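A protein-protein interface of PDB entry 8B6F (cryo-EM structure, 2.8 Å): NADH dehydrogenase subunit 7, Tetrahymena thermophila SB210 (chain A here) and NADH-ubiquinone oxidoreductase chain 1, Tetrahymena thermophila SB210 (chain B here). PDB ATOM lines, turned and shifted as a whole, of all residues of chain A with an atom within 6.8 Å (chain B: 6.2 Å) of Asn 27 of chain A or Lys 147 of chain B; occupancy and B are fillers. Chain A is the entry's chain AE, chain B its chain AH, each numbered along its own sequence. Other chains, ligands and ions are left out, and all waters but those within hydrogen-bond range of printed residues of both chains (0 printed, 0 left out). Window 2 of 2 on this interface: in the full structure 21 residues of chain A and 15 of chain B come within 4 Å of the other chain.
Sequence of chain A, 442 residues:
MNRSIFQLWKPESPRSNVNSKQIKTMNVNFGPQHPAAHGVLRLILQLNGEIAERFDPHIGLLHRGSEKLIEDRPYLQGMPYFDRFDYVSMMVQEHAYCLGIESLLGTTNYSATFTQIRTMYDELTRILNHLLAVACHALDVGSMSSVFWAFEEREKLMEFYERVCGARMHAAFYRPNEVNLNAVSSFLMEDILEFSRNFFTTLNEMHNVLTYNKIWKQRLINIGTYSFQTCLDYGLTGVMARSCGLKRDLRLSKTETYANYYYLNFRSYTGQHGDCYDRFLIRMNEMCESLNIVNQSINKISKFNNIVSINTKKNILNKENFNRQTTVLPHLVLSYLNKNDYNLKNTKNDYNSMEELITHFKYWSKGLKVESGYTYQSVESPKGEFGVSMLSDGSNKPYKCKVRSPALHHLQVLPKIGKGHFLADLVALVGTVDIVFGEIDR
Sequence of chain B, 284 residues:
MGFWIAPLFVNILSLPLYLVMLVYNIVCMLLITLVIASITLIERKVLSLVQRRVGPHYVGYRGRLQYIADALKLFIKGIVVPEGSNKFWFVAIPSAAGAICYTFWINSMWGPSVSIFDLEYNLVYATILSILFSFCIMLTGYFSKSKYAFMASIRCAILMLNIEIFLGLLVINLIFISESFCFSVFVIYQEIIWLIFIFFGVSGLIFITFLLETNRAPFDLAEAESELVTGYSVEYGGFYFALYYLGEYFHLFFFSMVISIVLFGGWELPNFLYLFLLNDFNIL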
ATOM      1  N   LYS A  24     -23.738  30.794  19.289  1.00  0.00           N
ATOM      2  CA  LYS A  24     -22.321  30.943  18.983  1.00  0.00           C
ATOM      3  C   LYS A  24     -21.699  29.551  18.965  1.00  0.00           C
ATOM      4  O   LYS A  24     -21.486  28.943  20.018  1.00  0.00           O
ATOM      5  CB  LYS A  24     -21.640  31.846  20.009  1.00  0.00           C
ATOM      6  CG  LYS A  24     -20.419  32.582  19.484  1.00  0.00           C
ATOM      7  CD  LYS A  24     -19.255  31.641  19.237  1.00  0.00           C
ATOM      8  CE  LYS A  24     -18.045  32.383  18.703  1.00  0.00           C
ATOM      9  NZ  LYS A  24     -18.292  32.942  17.350  1.00  0.00           N
ATOM     10  N   THR A  25     -21.413  29.048  17.768  1.00  0.00           N
ATOM     11  CA  THR A  25     -20.916  27.689  17.625  1.00  0.00           C
ATOM     12  C   THR A  25     -19.528  27.545  18.239  1.00  0.00           C
ATOM     13  O   THR A  25     -18.758  28.503  18.324  1.00  0.00           O
ATOM     14  CB  THR A  25     -20.873  27.296  16.149  1.00  0.00           C
ATOM     15  OG1 THR A  25     -20.031  28.209  15.433  1.00  0.00           O
ATOM     16  CG2 THR A  25     -22.270  27.324  15.550  1.00  0.00           C
ATOM     17  N   MET A  26     -19.216  26.327  18.674  1.00  0.00           N
ATOM     18  CA  MET A  26     -17.914  26.028  19.260  1.00  0.00           C
ATOM     19  C   MET A  26     -16.927  25.714  18.145  1.00  0.00           C
ATOM     20  O   MET A  26     -17.065  24.704  17.450  1.00  0.00           O
ATOM     21  CB  MET A  26     -18.013  24.854  20.231  1.00  0.00           C
ATOM     22  CG  MET A  26     -18.339  25.253  21.654  1.00  0.00           C
ATOM     23  SD  MET A  26     -18.268  23.854  22.784  1.00  0.00           S
ATOM     24  CE  MET A  26     -18.495  24.686  24.351  1.00  0.00           C
ATOM     25  N   ASN A  27     -15.931  26.575  17.973  1.00  0.00           N
ATOM     26  CA  ASN A  27     -14.869  26.374  16.991  1.00  0.00           C
ATOM     27  C   ASN A  27     -13.669  25.789  17.728  1.00  0.00           C
ATOM     28  O   ASN A  27     -12.864  26.525  18.305  1.00  0.00           O
ATOM     29  CB  ASN A  27     -14.525  27.681  16.293  1.00  0.00           C
ATOM     30  CG  ASN A  27     -15.692  28.252  15.517  1.00  0.00           C
ATOM     31  OD1 ASN A  27     -16.591  27.524  15.101  1.00  0.00           O
ATOM     32  ND2 ASN A  27     -15.683  29.563  15.317  1.00  0.00           N
ATOM     33  N   VAL A  28     -13.546  24.468  17.705  1.00  0.00           N
ATOM     34  CA  VAL A  28     -12.505  23.763  18.443  1.00  0.00           C
ATOM     35  C   VAL A  28     -11.389  23.376  17.485  1.00  0.00           C
ATOM     36  O   VAL A  28     -11.616  23.122  16.297  1.00  0.00           O
ATOM     37  CB  VAL A  28     -13.065  22.520  19.171  1.00  0.00           C
ATOM     38  CG1 VAL A  28     -14.156  22.920  20.144  1.00  0.00           C
ATOM     39  CG2 VAL A  28     -13.590  21.499  18.176  1.00  0.00           C
ATOM     40  N   ASN A  29     -10.165  23.336  18.009  1.00  0.00           N
ATOM     41  CA  ASN A  29      -8.997  22.888  17.252  1.00  0.00           C
ATOM     42  C   ASN A  29      -8.741  21.428  17.606  1.00  0.00           C
ATOM     43  O   ASN A  29      -7.888  21.095  18.427  1.00  0.00           O
ATOM     44  CB  ASN A  29      -7.782  23.758  17.554  1.00  0.00           C
ATOM     45  CG  ASN A  29      -7.878  25.135  16.934  1.00  0.00           C
ATOM     46  OD1 ASN A  29      -7.348  25.374  15.850  1.00  0.00           O
ATOM     47  ND2 ASN A  29      -8.555  26.048  17.618  1.00  0.00           N
ATOM     48  N   PHE A  30      -9.509  20.544  16.975  1.00  0.00           N
ATOM     49  CA  PHE A  30      -9.297  19.114  17.149  1.00  0.00           C
ATOM     50  C   PHE A  30      -7.898  18.761  16.661  1.00  0.00           C
ATOM     51  O   PHE A  30      -7.620  18.820  15.460  1.00  0.00           O
ATOM     52  CB  PHE A  30     -10.369  18.332  16.386  1.00  0.00           C
ATOM     53  CG  PHE A  30     -10.271  16.844  16.542  1.00  0.00           C
ATOM     54  CD1 PHE A  30     -10.902  16.203  17.595  1.00  0.00           C
ATOM     55  CD2 PHE A  30      -9.569  16.084  15.622  1.00  0.00           C
ATOM     56  CE1 PHE A  30     -10.820  14.830  17.736  1.00  0.00           C
ATOM     57  CE2 PHE A  30      -9.484  14.711  15.756  1.00  0.00           C
ATOM     58  CZ  PHE A  30     -10.112  14.083  16.814  1.00  0.00           C
ATOM     59  N   ILE A  44     -10.329  22.233  12.342  1.00  0.00           N
ATOM     60  CA  ILE A  44     -11.207  23.242  12.925  1.00  0.00           C
ATOM     61  C   ILE A  44     -12.628  22.699  12.844  1.00  0.00           C
ATOM     62  O   ILE A  44     -13.193  22.570  11.757  1.00  0.00           O
ATOM     63  CB  ILE A  44     -11.081  24.593  12.213  1.00  0.00           C
ATOM     64  CG1 ILE A  44      -9.612  24.922  11.929  1.00  0.00           C
ATOM     65  CG2 ILE A  44     -11.711  25.690  13.054  1.00  0.00           C
ATOM     66  CD1 ILE A  44      -8.711  24.847  13.148  1.00  0.00           C
ATOM     67  N   LEU A  45     -13.204  22.379  13.996  1.00  0.00           N
ATOM     68  CA  LEU A  45     -14.516  21.757  14.085  1.00  0.00           C
ATOM     69  C   LEU A  45     -15.533  22.768  14.589  1.00  0.00           C
ATOM     70  O   LEU A  45     -15.279  23.471  15.572  1.00  0.00           O
ATOM     71  CB  LEU A  45     -14.473  20.551  15.020  1.00  0.00           C
ATOM     72  CG  LEU A  45     -14.340  19.174  14.382  1.00  0.00           C
ATOM     73  CD1 LEU A  45     -14.115  18.142  15.462  1.00  0.00           C
ATOM     74  CD2 LEU A  45     -15.571  18.831  13.567  1.00  0.00           C
ATOM     75  N   GLN A  46     -16.677  22.839  13.916  1.00  0.00           N
ATOM     76  CA  GLN A  46     -17.785  23.694  14.329  1.00  0.00           C
ATOM     77  C   GLN A  46     -18.828  22.803  14.995  1.00  0.00           C
ATOM     78  O   GLN A  46     -19.669  22.202  14.323  1.00  0.00           O
ATOM     79  CB  GLN A  46     -18.369  24.444  13.138  1.00  0.00           C
ATOM     80  CG  GLN A  46     -19.554  25.325  13.490  1.00  0.00           C
ATOM     81  CD  GLN A  46     -20.115  26.045  12.285  1.00  0.00           C
ATOM     82  OE1 GLN A  46     -19.375  26.455  11.394  1.00  0.00           O
ATOM     83  NE2 GLN A  46     -21.433  26.192  12.246  1.00  0.00           N
ATOM     84  N   LEU A  47     -18.770  22.722  16.321  1.00  0.00           N
ATOM     85  CA  LEU A  47     -19.721  21.938  17.094  1.00  0.00           C
ATOM     86  C   LEU A  47     -20.910  22.793  17.500  1.00  0.00           C
ATOM     87  O   LEU A  47     -20.761  23.970  17.840  1.00  0.00           O
ATOM     88  CB  LEU A  47     -19.054  21.353  18.340  1.00  0.00           C
ATOM     89  CG  LEU A  47     -18.395  19.982  18.180  1.00  0.00           C
ATOM     90  CD1 LEU A  47     -17.411  19.979  17.034  1.00  0.00           C
ATOM     91  CD2 LEU A  47     -17.704  19.579  19.467  1.00  0.00           C
ATOM     92  N   SER B 144     -12.581  26.480  34.100  1.00  0.00           N
ATOM     93  CA  SER B 144     -11.477  26.232  33.181  1.00  0.00           C
ATOM     94  C   SER B 144     -12.044  26.375  31.775  1.00  0.00           C
ATOM     95  O   SER B 144     -12.773  25.498  31.301  1.00  0.00           O
ATOM     96  CB  SER B 144     -10.871  24.850  33.405  1.00  0.00           C
ATOM     97  OG  SER B 144     -11.823  23.828  33.167  1.00  0.00           O
ATOM     98  N   LYS B 145     -11.712  27.470  31.109  1.00  0.00           N
ATOM     99  CA  LYS B 145     -12.415  27.846  29.884  1.00  0.00           C
ATOM    100  C   LYS B 145     -12.096  26.958  28.712  1.00  0.00           C
ATOM    101  O   LYS B 145     -12.513  27.298  27.598  1.00  0.00           O
ATOM    102  CB  LYS B 145     -12.099  29.300  29.534  1.00  0.00           C
ATOM    103  CG  LYS B 145     -12.605  30.304  30.558  1.00  0.00           C
ATOM    104  CD  LYS B 145     -14.126  30.300  30.642  1.00  0.00           C
ATOM    105  CE  LYS B 145     -14.627  31.310  31.656  1.00  0.00           C
ATOM    106  NZ  LYS B 145     -16.108  31.252  31.802  1.00  0.00           N
ATOM    107  N   SER B 146     -11.388  25.847  28.884  1.00  0.00           N
ATOM    108  CA  SER B 146     -11.175  24.930  27.777  1.00  0.00           C
ATOM    109  C   SER B 146     -12.512  24.440  27.241  1.00  0.00           C
ATOM    110  O   SER B 146     -13.399  24.053  28.004  1.00  0.00           O
ATOM    111  CB  SER B 146     -10.317  23.747  28.220  1.00  0.00           C
ATOM    112  OG  SER B 146     -10.110  22.857  27.136  1.00  0.00           O
ATOM    113  N   LYS B 147     -12.656  24.470  25.916  1.00  0.00           N
ATOM    114  CA  LYS B 147     -13.884  23.984  25.299  1.00  0.00           C
ATOM    115  C   LYS B 147     -14.079  22.499  25.570  1.00  0.00           C
ATOM    116  O   LYS B 147     -15.207  22.044  25.794  1.00  0.00           O
ATOM    117  CB  LYS B 147     -13.857  24.263  23.797  1.00  0.00           C
ATOM    118  CG  LYS B 147     -13.755  25.742  23.454  1.00  0.00           C
ATOM    119  CD  LYS B 147     -13.621  25.958  21.957  1.00  0.00           C
ATOM    120  CE  LYS B 147     -13.486  27.432  21.619  1.00  0.00           C
ATOM    121  NZ  LYS B 147     -14.700  28.202  21.992  1.00  0.00           N
ATOM    122  N   TYR B 148     -12.992  21.727  25.556  1.00  0.00           N
ATOM    123  CA  TYR B 148     -13.092  20.309  25.886  1.00  0.00           C
ATOM    124  C   TYR B 148     -13.567  20.110  27.320  1.00  0.00           C
ATOM    125  O   TYR B 148     -14.406  19.242  27.589  1.00  0.00           O
ATOM    126  CB  TYR B 148     -11.744  19.625  25.669  1.00  0.00           C
ATOM    127  CG  TYR B 148     -11.255  19.692  24.243  1.00  0.00           C
ATOM    128  CD1 TYR B 148     -11.771  18.842  23.272  1.00  0.00           C
ATOM    129  CD2 TYR B 148     -10.279  20.602  23.865  1.00  0.00           C
ATOM    130  CE1 TYR B 148     -11.328  18.897  21.965  1.00  0.00           C
ATOM    131  CE2 TYR B 148      -9.830  20.665  22.560  1.00  0.00           C
ATOM    132  CZ  TYR B 148     -10.358  19.811  21.615  1.00  0.00           C
ATOM    133  OH  TYR B 148      -9.915  19.869  20.316  1.00  0.00           O
ATOM    134  N   ALA B 149     -13.038  20.899  28.256  1.00  0.00           N
ATOM    135  CA  ALA B 149     -13.482  20.799  29.641  1.00  0.00           C
ATOM    136  C   ALA B 149     -14.953  21.159  29.777  1.00  0.00           C
ATOM    137  O   ALA B 149     -15.689  20.521  30.538  1.00  0.00           O
ATOM    138  CB  ALA B 149     -12.639  21.709  30.531  1.00  0.00           C
ATOM    139  N   PHE B 150     -15.402  22.184  29.054  1.00  0.00           N
ATOM    140  CA  PHE B 150     -16.803  22.573  29.132  1.00  0.00           C
ATOM    141  C   PHE B 150     -17.705  21.490  28.554  1.00  0.00           C
ATOM    142  O   PHE B 150     -18.770  21.203  29.110  1.00  0.00           O
ATOM    143  CB  PHE B 150     -17.013  23.908  28.418  1.00  0.00           C
ATOM    144  CG  PHE B 150     -18.264  24.623  28.832  1.00  0.00           C
ATOM    145  CD1 PHE B 150     -18.572  24.793  30.171  1.00  0.00           C
ATOM    146  CD2 PHE B 150     -19.119  25.154  27.885  1.00  0.00           C
ATOM    147  CE1 PHE B 150     -19.714  25.455  30.554  1.00  0.00           C
ATOM    148  CE2 PHE B 150     -20.265  25.820  28.267  1.00  0.00           C
ATOM    149  CZ  PHE B 150     -20.561  25.971  29.601  1.00  0.00           C
ATOM    150  N   MET B 151     -17.297  20.874  27.443  1.00  0.00           N
ATOM    151  CA  MET B 151     -18.065  19.756  26.903  1.00  0.00           C
ATOM    152  C   MET B 151     -18.089  18.589  27.882  1.00  0.00           C
ATOM    153  O   MET B 151     -19.107  17.903  28.020  1.00  0.00           O
ATOM    154  CB  MET B 151     -17.492  19.319  25.556  1.00  0.00           C
ATOM    155  CG  MET B 151     -17.763  20.306  24.433  1.00  0.00           C
ATOM    156  SD  MET B 151     -17.216  19.728  22.816  1.00  0.00           S
ATOM    157  CE  MET B 151     -15.443  19.660  23.049  1.00  0.00           C
ATOM    158  N   ALA B 152     -16.976  18.355  28.578  1.00  0.00           N
ATOM    159  CA  ALA B 152     -16.950  17.322  29.608  1.00  0.00           C
ATOM    160  C   ALA B 152     -17.927  17.642  30.731  1.00  0.00           C
ATOM    161  O   ALA B 152     -18.578  16.742  31.273  1.00  0.00           O
ATOM    162  CB  ALA B 152     -15.535  17.170  30.164  1.00  0.00           C
ATOM    163  N   LEU B 228     -12.369  13.494  24.285  1.00  0.00           N
ATOM    164  CA  LEU B 228     -11.850  14.749  24.801  1.00  0.00           C
ATOM    165  C   LEU B 228     -10.407  14.539  25.237  1.00  0.00           C
ATOM    166  O   LEU B 228      -9.969  13.410  25.468  1.00  0.00           O
ATOM    167  CB  LEU B 228     -12.697  15.257  25.974  1.00  0.00           C
ATOM    168  CG  LEU B 228     -14.197  15.365  25.687  1.00  0.00           C
ATOM    169  CD1 LEU B 228     -14.959  15.714  26.947  1.00  0.00           C
ATOM    170  CD2 LEU B 228     -14.469  16.393  24.604  1.00  0.00           C
ATOM    171  N   GLU B 235      -7.147  21.284  32.172  1.00  0.00           N
ATOM    172  CA  GLU B 235      -6.296  22.414  32.528  1.00  0.00           C
ATOM    173  C   GLU B 235      -5.866  22.388  33.988  1.00  0.00           C
ATOM    174  O   GLU B 235      -5.378  23.404  34.495  1.00  0.00           O
ATOM    175  CB  GLU B 235      -7.007  23.735  32.222  1.00  0.00           C
ATOM    176  CG  GLU B 235      -7.081  24.052  30.739  1.00  0.00           C
ATOM    177  CD  GLU B 235      -7.824  25.337  30.452  1.00  0.00           C
ATOM    178  OE1 GLU B 235      -8.462  25.873  31.382  1.00  0.00           O
ATOM    179  OE2 GLU B 235      -7.772  25.810  29.298  1.00  0.00           O
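OH of Tyr 148 of chain B sits at hydrogen-bond distance from O of Asn 29 of chain A (3.0 Å).
The side-chain hydroxyl of Tyr 148 of chain B sits close to the backbone NH of Phe 30 of chain A, at 3.4 Å.
The backbone carbonyl oxygen (O) of Val 28 of chain A lies within hydrogen-bond range of the backbone NH (N) of Leu 45 of chain A (2.9 Å).
O of Met 26 of chain A sits at hydrogen-bond distance from N of Leu 47 of chain A.
OG of Ser 146 of chain B sits close to N of Tyr 148 of chain B (3.5 Å).
Met 26 of chain A touches Phe 150 of chain B.
Met 26 of chain A touches Met 151 of chain B.
CE of Lys 147 of chain B touches O of Asn 27 of chain A, 3.5 Å away.
Val 28 of chain A touches Lys 147 of chain B.
SD of Met 151 of chain B touches CD2 of Leu 47 of chain A, at 3.4 Å.
Printed residues of chain B within 4 Å of Met 26 of chain A: Phe 150 and Met 151.
Of the printed residues of chain B, Leu 47 of chain A touches Met 151.
Lys 147 of chain B touches just these residues of chain A: Asn 27 and Val 28.
Printed residues of chain A within 4 Å of Met 151 of chain B: Met 26 and Leu 47.
The nearest printed residue of chain B that does not touch Asn 27 of chain A is Tyr 148 of chain B (7.5 Å).
The nearest residue of chain A that does not touch Lys 147 of chain B is Met 26 of chain A (4.5 Å).
The nearest printed residue of chain B that does not touch Asn 29 of chain A is Lys 147 of chain B (5.9 Å).
Hydrophobic or aromatic side chains of chain A within 4 Å of the printed part of chain B: Met 26, Val 28 and Leu 47.
Of the 11 printed residues of chain B, 4 touch a printed residue of chain A.
Hydrophobic or aromatic side chains of chain B that line the printed part of chain A: Tyr 148, Phe 150 and Met 151.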
